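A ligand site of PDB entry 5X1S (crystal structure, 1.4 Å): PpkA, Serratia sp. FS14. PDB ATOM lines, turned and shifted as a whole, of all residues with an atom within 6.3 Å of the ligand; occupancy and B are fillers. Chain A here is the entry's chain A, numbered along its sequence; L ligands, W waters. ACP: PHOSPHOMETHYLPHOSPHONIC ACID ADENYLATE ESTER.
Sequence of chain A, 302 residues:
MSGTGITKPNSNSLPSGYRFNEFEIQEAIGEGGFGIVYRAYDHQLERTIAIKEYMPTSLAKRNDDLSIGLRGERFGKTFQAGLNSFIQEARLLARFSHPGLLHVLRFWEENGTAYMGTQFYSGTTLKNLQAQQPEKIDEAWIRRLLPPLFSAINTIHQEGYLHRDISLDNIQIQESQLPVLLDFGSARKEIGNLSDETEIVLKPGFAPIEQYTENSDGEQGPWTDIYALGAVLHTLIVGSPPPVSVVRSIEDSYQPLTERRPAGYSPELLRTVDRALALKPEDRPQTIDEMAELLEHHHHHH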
ATOM      1  N   ILE A  29      20.434  35.294  19.609  1.00  0.00           N
ATOM      2  CA  ILE A  29      20.836  34.623  20.836  1.00  0.00           C
ATOM      3  C   ILE A  29      22.338  34.489  20.962  1.00  0.00           C
ATOM      4  O   ILE A  29      22.841  34.142  22.049  1.00  0.00           O
ATOM      5  CB  ILE A  29      20.162  33.245  20.984  1.00  0.00           C
ATOM      6  CG1 ILE A  29      20.542  32.321  19.813  1.00  0.00           C
ATOM      7  CG2 ILE A  29      18.654  33.433  21.108  1.00  0.00           C
ATOM      8  CD1 ILE A  29      19.999  30.906  19.954  1.00  0.00           C
ATOM      9  N   GLY A  30      23.085  34.717  19.892  1.00  0.00           N
ATOM     10  CA  GLY A  30      24.526  34.695  19.962  1.00  0.00           C
ATOM     11  C   GLY A  30      25.077  35.759  19.040  1.00  0.00           C
ATOM     12  O   GLY A  30      24.613  35.906  17.910  1.00  0.00           O
ATOM     13  N   GLU A  31      26.038  36.531  19.514  1.00  0.00           N
ATOM     14  CA  GLU A  31      26.658  37.548  18.669  1.00  0.00           C
ATOM     15  C   GLU A  31      28.134  37.595  19.035  1.00  0.00           C
ATOM     16  O   GLU A  31      28.503  38.095  20.100  1.00  0.00           O
ATOM     17  CB  GLU A  31      25.988  38.912  18.825  1.00  0.00           C
ATOM     18  CG  GLU A  31      26.573  39.948  17.877  1.00  0.00           C
ATOM     19  CD  GLU A  31      25.639  41.118  17.652  1.00  0.00           C
ATOM     20  OE1 GLU A  31      24.679  41.267  18.444  1.00  0.00           O
ATOM     21  OE2 GLU A  31      25.850  41.873  16.668  1.00  0.00           O
ATOM     22  N   GLY A  32      28.963  37.059  18.151  1.00  0.00           N
ATOM     23  CA  GLY A  32      30.386  37.086  18.352  1.00  0.00           C
ATOM     24  C   GLY A  32      31.074  37.853  17.240  1.00  0.00           C
ATOM     25  O   GLY A  32      30.419  38.498  16.408  1.00  0.00           O
ATOM     26  N   GLY A  33      32.404  37.775  17.214  1.00  0.00           N
ATOM     27  CA  GLY A  33      33.128  38.531  16.226  1.00  0.00           C
ATOM     28  C   GLY A  33      32.958  38.042  14.814  1.00  0.00           C
ATOM     29  O   GLY A  33      33.336  38.758  13.883  1.00  0.00           O
ATOM     30  N   GLY A  35      30.076  35.740  13.613  1.00  0.00           N
ATOM     31  CA  GLY A  35      28.763  35.326  13.167  1.00  0.00           C
ATOM     32  C   GLY A  35      27.740  35.654  14.224  1.00  0.00           C
ATOM     33  O   GLY A  35      28.062  35.895  15.389  1.00  0.00           O
ATOM     34  N   VAL A  37      23.975  34.189  15.745  1.00  0.00           N
ATOM     35  CA  VAL A  37      23.042  33.069  15.818  1.00  0.00           C
ATOM     36  C   VAL A  37      21.683  33.611  16.245  1.00  0.00           C
ATOM     37  O   VAL A  37      21.594  34.342  17.240  1.00  0.00           O
ATOM     38  CB  VAL A  37      23.498  31.993  16.812  1.00  0.00           C
ATOM     39  CG1 VAL A  37      22.512  30.813  16.839  1.00  0.00           C
ATOM     40  CG2 VAL A  37      24.904  31.509  16.459  1.00  0.00           C
ATOM     41  N   ALA A  50      17.431  27.296  14.369  1.00  0.00           N
ATOM     42  CA  ALA A  50      18.432  28.342  14.509  1.00  0.00           C
ATOM     43  C   ALA A  50      18.900  28.769  13.130  1.00  0.00           C
ATOM     44  O   ALA A  50      18.904  27.974  12.186  1.00  0.00           O
ATOM     45  CB  ALA A  50      19.642  27.874  15.314  1.00  0.00           C
ATOM     46  N   LYS A  52      22.306  30.712  11.512  1.00  0.00           N
ATOM     47  CA  LYS A  52      23.633  31.231  11.723  1.00  0.00           C
ATOM     48  C   LYS A  52      23.978  32.117  10.521  1.00  0.00           C
ATOM     49  O   LYS A  52      23.923  31.677   9.432  1.00  0.00           O
ATOM     50  CB  LYS A  52      24.602  30.067  11.796  1.00  0.00           C
ATOM     51  CG  LYS A  52      25.870  30.362  12.472  1.00  0.00           C
ATOM     52  CD  LYS A  52      26.379  31.638  11.991  1.00  0.00           C
ATOM     53  CE  LYS A  52      27.148  32.332  13.053  1.00  0.00           C
ATOM     54  NZ  LYS A  52      26.964  31.808  14.386  1.00  0.00           N
ATOM     55  N   LEU A 102      25.903  19.326  15.236  1.00  0.00           N
ATOM     56  CA  LEU A 102      24.949  20.328  14.754  1.00  0.00           C
ATOM     57  C   LEU A 102      24.303  19.863  13.463  1.00  0.00           C
ATOM     58  O   LEU A 102      24.998  19.608  12.469  1.00  0.00           O
ATOM     59  CB  LEU A 102      25.701  21.633  14.505  1.00  0.00           C
ATOM     60  CG  LEU A 102      24.885  22.812  13.940  1.00  0.00           C
ATOM     61  CD1 LEU A 102      24.273  23.601  15.062  1.00  0.00           C
ATOM     62  CD2 LEU A 102      25.800  23.717  13.120  1.00  0.00           C
ATOM     63  N   THR A 118      19.637  25.587  10.962  1.00  0.00           N
ATOM     64  CA  THR A 118      20.033  24.377  11.691  1.00  0.00           C
ATOM     65  C   THR A 118      18.972  24.011  12.720  1.00  0.00           C
ATOM     66  O   THR A 118      18.061  24.804  13.026  1.00  0.00           O
ATOM     67  CB  THR A 118      21.383  24.520  12.434  1.00  0.00           C
ATOM     68  OG1 THR A 118      21.203  25.296  13.638  1.00  0.00           O
ATOM     69  CG2 THR A 118      22.435  25.196  11.567  1.00  0.00           C
ATOM     70  N   GLN A 119      19.093  22.801  13.257  1.00  0.00           N
ATOM     71  CA  GLN A 119      18.291  22.435  14.408  1.00  0.00           C
ATOM     72  C   GLN A 119      18.539  23.429  15.536  1.00  0.00           C
ATOM     73  O   GLN A 119      19.658  23.942  15.704  1.00  0.00           O
ATOM     74  CB  GLN A 119      18.680  21.026  14.842  1.00  0.00           C
ATOM     75  CG  GLN A 119      17.816  20.446  15.940  1.00  0.00           C
ATOM     76  CD  GLN A 119      17.968  18.953  16.085  1.00  0.00           C
ATOM     77  OE1 GLN A 119      18.257  18.256  15.105  1.00  0.00           O
ATOM     78  NE2 GLN A 119      17.788  18.450  17.291  1.00  0.00           N
ATOM     79  N   PHE A 120      17.483  23.725  16.304  1.00  0.00           N
ATOM     80  CA  PHE A 120      17.580  24.583  17.474  1.00  0.00           C
ATOM     81  C   PHE A 120      17.702  23.694  18.713  1.00  0.00           C
ATOM     82  O   PHE A 120      16.853  22.819  18.922  1.00  0.00           O
ATOM     83  CB  PHE A 120      16.348  25.489  17.603  1.00  0.00           C
ATOM     84  CG  PHE A 120      16.378  26.353  18.829  1.00  0.00           C
ATOM     85  CD1 PHE A 120      17.093  27.524  18.852  1.00  0.00           C
ATOM     86  CD2 PHE A 120      15.706  25.949  19.974  1.00  0.00           C
ATOM     87  CE1 PHE A 120      17.136  28.298  20.026  1.00  0.00           C
ATOM     88  CE2 PHE A 120      15.735  26.723  21.106  1.00  0.00           C
ATOM     89  CZ  PHE A 120      16.443  27.884  21.136  1.00  0.00           C
ATOM     90  N   TYR A 121      18.743  23.907  19.511  1.00  0.00           N
ATOM     91  CA  TYR A 121      18.999  23.077  20.680  1.00  0.00           C
ATOM     92  C   TYR A 121      18.614  23.793  21.961  1.00  0.00           C
ATOM     93  O   TYR A 121      18.809  25.001  22.102  1.00  0.00           O
ATOM     94  CB  TYR A 121      20.469  22.635  20.747  1.00  0.00           C
ATOM     95  CG  TYR A 121      20.841  21.826  19.536  1.00  0.00           C
ATOM     96  CD1 TYR A 121      20.508  20.471  19.450  1.00  0.00           C
ATOM     97  CD2 TYR A 121      21.467  22.420  18.457  1.00  0.00           C
ATOM     98  CE1 TYR A 121      20.798  19.744  18.320  1.00  0.00           C
ATOM     99  CE2 TYR A 121      21.768  21.695  17.340  1.00  0.00           C
ATOM    100  CZ  TYR A 121      21.443  20.362  17.274  1.00  0.00           C
ATOM    101  OH  TYR A 121      21.750  19.653  16.143  1.00  0.00           O
ATOM    102  N   SER A 122      18.063  23.025  22.909  1.00  0.00           N
ATOM    103  CA  SER A 122      17.807  23.549  24.246  1.00  0.00           C
ATOM    104  C   SER A 122      19.123  23.750  24.986  1.00  0.00           C
ATOM    105  O   SER A 122      20.202  23.389  24.512  1.00  0.00           O
ATOM    106  CB  SER A 122      16.947  22.570  25.031  1.00  0.00           C
ATOM    107  OG  SER A 122      17.635  21.354  25.274  1.00  0.00           O
ATOM    108  N   GLY A 123      19.033  24.343  26.178  1.00  0.00           N
ATOM    109  CA  GLY A 123      20.214  24.454  27.017  1.00  0.00           C
ATOM    110  C   GLY A 123      21.068  25.655  26.641  1.00  0.00           C
ATOM    111  O   GLY A 123      20.592  26.646  26.081  1.00  0.00           O
ATOM    112  N   THR A 124      22.358  25.548  26.967  1.00  0.00           N
ATOM    113  CA  THR A 124      23.331  26.605  26.655  1.00  0.00           C
ATOM    114  C   THR A 124      24.702  25.947  26.502  1.00  0.00           C
ATOM    115  O   THR A 124      24.817  24.726  26.556  1.00  0.00           O
ATOM    116  CB  THR A 124      23.294  27.700  27.715  1.00  0.00           C
ATOM    117  OG1 THR A 124      24.064  28.821  27.254  1.00  0.00           O
ATOM    118  CG2 THR A 124      23.864  27.199  29.034  1.00  0.00           C
ATOM    119  N   THR A 125      25.742  26.761  26.328  1.00  0.00           N
ATOM    120  CA  THR A 125      27.066  26.197  26.110  1.00  0.00           C
ATOM    121  C   THR A 125      27.660  25.673  27.412  1.00  0.00           C
ATOM    122  O   THR A 125      27.301  26.090  28.523  1.00  0.00           O
ATOM    123  CB  THR A 125      28.028  27.240  25.550  1.00  0.00           C
ATOM    124  OG1 THR A 125      28.172  28.298  26.498  1.00  0.00           O
ATOM    125  CG2 THR A 125      27.534  27.758  24.209  1.00  0.00           C
ATOM    126  N   LYS A 127      30.613  26.343  28.374  1.00  0.00           N
ATOM    127  CA  LYS A 127      31.252  27.519  28.973  1.00  0.00           C
ATOM    128  C   LYS A 127      30.281  28.255  29.889  1.00  0.00           C
ATOM    129  O   LYS A 127      30.635  28.620  31.024  1.00  0.00           O
ATOM    130  CB  LYS A 127      31.751  28.449  27.855  1.00  0.00           C
ATOM    131  CG  LYS A 127      32.209  29.831  28.327  1.00  0.00           C
ATOM    132  CD  LYS A 127      32.740  30.632  27.154  1.00  0.00           C
ATOM    133  CE  LYS A 127      32.483  32.120  27.290  1.00  0.00           C
ATOM    134  NZ  LYS A 127      33.711  32.920  27.011  1.00  0.00           N
ATOM    135  N   ASN A 128      29.048  28.466  29.431  1.00  0.00           N
ATOM    136  CA  ASN A 128      28.074  29.175  30.262  1.00  0.00           C
ATOM    137  C   ASN A 128      27.658  28.332  31.472  1.00  0.00           C
ATOM    138  O   ASN A 128      27.467  28.865  32.560  1.00  0.00           O
ATOM    139  CB  ASN A 128      26.838  29.566  29.444  1.00  0.00           C
ATOM    140  CG  ASN A 128      27.121  30.711  28.487  1.00  0.00           C
ATOM    141  OD1 ASN A 128      28.108  31.437  28.624  1.00  0.00           O
ATOM    142  ND2 ASN A 128      26.236  30.879  27.516  1.00  0.00           N
ATOM    143  N   GLN A 132      27.977  29.585  35.284  1.00  0.00           N
ATOM    144  CA  GLN A 132      26.747  29.861  36.014  1.00  0.00           C
ATOM    145  C   GLN A 132      26.423  28.804  37.062  1.00  0.00           C
ATOM    146  O   GLN A 132      25.914  29.140  38.137  1.00  0.00           O
ATOM    147  CB  GLN A 132      25.576  29.968  35.029  1.00  0.00           C
ATOM    148  CG  GLN A 132      25.676  31.147  34.063  1.00  0.00           C
ATOM    149  CD  GLN A 132      24.884  30.933  32.784  1.00  0.00           C
ATOM    150  OE1 GLN A 132      24.101  29.990  32.680  1.00  0.00           O
ATOM    151  NE2 GLN A 132      25.090  31.810  31.810  1.00  0.00           N
ATOM    152  N   ASP A 169      33.534  26.586  24.618  1.00  0.00           N
ATOM    153  CA  ASP A 169      32.686  27.608  24.004  1.00  0.00           C
ATOM    154  C   ASP A 169      31.741  27.027  22.970  1.00  0.00           C
ATOM    155  O   ASP A 169      30.648  27.563  22.758  1.00  0.00           O
ATOM    156  CB  ASP A 169      33.562  28.679  23.368  1.00  0.00           C
ATOM    157  CG  ASP A 169      34.446  29.393  24.383  1.00  0.00           C
ATOM    158  OD1 ASP A 169      34.679  28.822  25.473  1.00  0.00           O
ATOM    159  OD2 ASP A 169      34.892  30.518  24.091  1.00  0.00           O
ATOM    160  N   GLN A 172      27.401  22.578  23.102  1.00  0.00           N
ATOM    161  CA  GLN A 172      26.104  22.865  23.704  1.00  0.00           C
ATOM    162  C   GLN A 172      25.767  21.750  24.696  1.00  0.00           C
ATOM    163  O   GLN A 172      25.994  20.572  24.419  1.00  0.00           O
ATOM    164  CB  GLN A 172      25.033  22.896  22.622  1.00  0.00           C
ATOM    165  CG  GLN A 172      23.639  23.334  23.101  1.00  0.00           C
ATOM    166  CD  GLN A 172      23.474  24.844  23.171  1.00  0.00           C
ATOM    167  OE1 GLN A 172      24.421  25.596  22.963  1.00  0.00           O
ATOM    168  NE2 GLN A 172      22.256  25.290  23.468  1.00  0.00           N
ATOM    169  N   LEU A 182      28.835  22.401  18.080  1.00  0.00           N
ATOM    170  CA  LEU A 182      28.124  23.456  17.367  1.00  0.00           C
ATOM    171  C   LEU A 182      28.879  24.080  16.203  1.00  0.00           C
ATOM    172  O   LEU A 182      28.241  24.673  15.326  1.00  0.00           O
ATOM    173  CB  LEU A 182      27.815  24.613  18.314  1.00  0.00           C
ATOM    174  CG  LEU A 182      26.854  24.365  19.462  1.00  0.00           C
ATOM    175  CD1 LEU A 182      26.847  25.550  20.413  1.00  0.00           C
ATOM    176  CD2 LEU A 182      25.457  24.060  18.920  1.00  0.00           C
HETATM  177  PG  ACP L   1      26.576  33.254  24.966  1.00  0.00           P
HETATM  178  O1G ACP L   1      28.063  32.955  24.394  1.00  0.00           O
HETATM  179  O2G ACP L   1      25.831  31.986  25.059  1.00  0.00           O
HETATM  180  O3G ACP L   1      26.658  33.932  26.426  1.00  0.00           O
HETATM  181  PB  ACP L   1      27.000  35.345  22.950  1.00  0.00           P
HETATM  182  O1B ACP L   1      28.332  35.530  23.816  1.00  0.00           O
HETATM  183  O2B ACP L   1      26.421  36.642  22.533  1.00  0.00           O
HETATM  184  C3B ACP L   1      25.740  34.414  23.855  1.00  0.00           C
HETATM  185  PA  ACP L   1      28.403  33.528  21.139  1.00  0.00           P
HETATM  186  O1A ACP L   1      29.647  33.637  21.985  1.00  0.00           O
HETATM  187  O2A ACP L   1      28.644  33.880  19.698  1.00  0.00           O
HETATM  188  O3A ACP L   1      27.254  34.570  21.560  1.00  0.00           O
HETATM  189  O5' ACP L   1      27.868  32.014  21.249  1.00  0.00           O
HETATM  190  C5' ACP L   1      26.864  31.501  20.393  1.00  0.00           C
HETATM  191  C4' ACP L   1      25.579  31.299  21.178  1.00  0.00           C
HETATM  192  O4' ACP L   1      24.621  30.702  20.294  1.00  0.00           O
HETATM  193  C3' ACP L   1      25.728  30.352  22.363  1.00  0.00           C
HETATM  194  O3' ACP L   1      24.976  30.830  23.473  1.00  0.00           O
HETATM  195  C2' ACP L   1      25.094  29.071  21.889  1.00  0.00           C
HETATM  196  O2' ACP L   1      24.438  28.370  22.956  1.00  0.00           O
HETATM  197  C1' ACP L   1      24.058  29.554  20.910  1.00  0.00           C
HETATM  198  N9  ACP L   1      23.772  28.609  19.816  1.00  0.00           N
HETATM  199  C8  ACP L   1      24.553  28.396  18.749  1.00  0.00           C
HETATM  200  N7  ACP L   1      23.987  27.490  17.919  1.00  0.00           N
HETATM  201  C5  ACP L   1      22.803  27.138  18.471  1.00  0.00           C
HETATM  202  C6  ACP L   1      21.694  26.244  18.096  1.00  0.00           C
HETATM  203  N6  ACP L   1      21.787  25.525  16.965  1.00  0.00           N
HETATM  204  N1  ACP L   1      20.639  26.140  18.936  1.00  0.00           N
HETATM  205  C2  ACP L   1      20.579  26.857  20.085  1.00  0.00           C
HETATM  206  N3  ACP L   1      21.544  27.713  20.481  1.00  0.00           N
HETATM  207  C4  ACP L   1      22.666  27.878  19.727  1.00  0.00           C
HETATM  208  O   HOH W   1      21.229  28.278  23.253  1.00  0.00           O
HETATM  209  O   HOH W   2      27.625  29.054  17.281  1.00  0.00           O
HETATM  210  O   HOH W   3      29.058  29.033  21.255  1.00  0.00           O
HETATM  211  O   HOH W   4      26.341  27.105  16.075  1.00  0.00           O
HETATM  212  O   HOH W   5      22.874  29.771  24.933  1.00  0.00           O
HETATM  213  O   HOH W   6      27.561  33.841  17.336  1.00  0.00           O
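Ile 29 touches the ligand (O to C3B, 3.4 Å). Gly 30 touches the ligand. N of Gly 32 touches O2A of the ligand, at 3.5 Å. Val 37 touches the ligand (CG1 to C8, 3.7 Å). Ala 50 touches the ligand (CB to N6, 3.6 Å). CD1 of Leu 102 touches N6 of the ligand, at 3.7 Å. Phe 120 touches the ligand (CA to N1, 3.7 Å). Thr 125 touches the ligand. Leu 182 touches the ligand.
The backbone carbonyl oxygen of Gly 123 sits at hydrogen-bond distance from the side-chain amide nitrogen of Gln 172 (3.4 Å). The backbone carbonyl oxygen (O) of Gly 30 sits at hydrogen-bond distance from the backbone NH (N) of Val 37, 2.8 Å away. The backbone NH of Thr 118 is in hydrogen-bond range of the backbone carbonyl oxygen of Ala 50. N of Asn 128 is in hydrogen-bond range of OG1 of Thr 125, 3.1 Å away. The side-chain hydroxyl (OG1) of Thr 124 lies within hydrogen-bond range of the side-chain amide nitrogen (ND2) of Asn 128 (3.0 Å). The backbone NH (N) of Ile 29 lies within hydrogen-bond range of the backbone carbonyl oxygen (O) of Val 37, 2.8 Å away. NE2 of Gln 172 lies within hydrogen-bond range of O of Ser 122 (3.0 Å).
Water W6 lies within hydrogen-bond range of an oxygen (O2A) of the ligand and the backbone carbonyl oxygen (O) of Gly 35. Water W5 lies within hydrogen-bond range of an oxygen (O3') of the ligand (2.8 Å) and the side-chain hydroxyl of Thr 124 (2.8 Å). Water W1 lies within hydrogen-bond range of a nitrogen (N3) of the ligand (2.8 Å), the side-chain amide nitrogen of Gln 172 (3.2 Å) and the backbone carbonyl oxygen of Gly 123 (3.3 Å). Water W4 lies within hydrogen-bond range of a nitrogen (N7) of the ligand (3.0 Å) and the backbone carbonyl oxygen (O) of Leu 182 (3.2 Å). Water W3 lies within hydrogen-bond range of the backbone carbonyl oxygen (O) of Asp 169 (2.6 Å) and an oxygen (O5') of the ligand (3.2 Å).
An oxygen (O2G) of the ligand sits at hydrogen-bond distance from the side-chain amide nitrogen (ND2) of Asn 128 (2.7 Å). The side-chain hydroxyl (OG1) of Thr 118 sits at hydrogen-bond distance from a nitrogen (N6) of the ligand (3.4 Å). The backbone NH (N) of Tyr 121 lies within hydrogen-bond range of a nitrogen (N1) of the ligand (3.0 Å). The side-chain amide oxygen (OE1) of Gln 172 sits at hydrogen-bond distance from an oxygen (O2') of the ligand (2.8 Å). The backbone carbonyl oxygen (O) of Gln 119 sits at hydrogen-bond distance from a nitrogen (N6) of the ligand. N of Glu 31 is in hydrogen-bond range of O2B of the ligand, at 3.0 Å.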
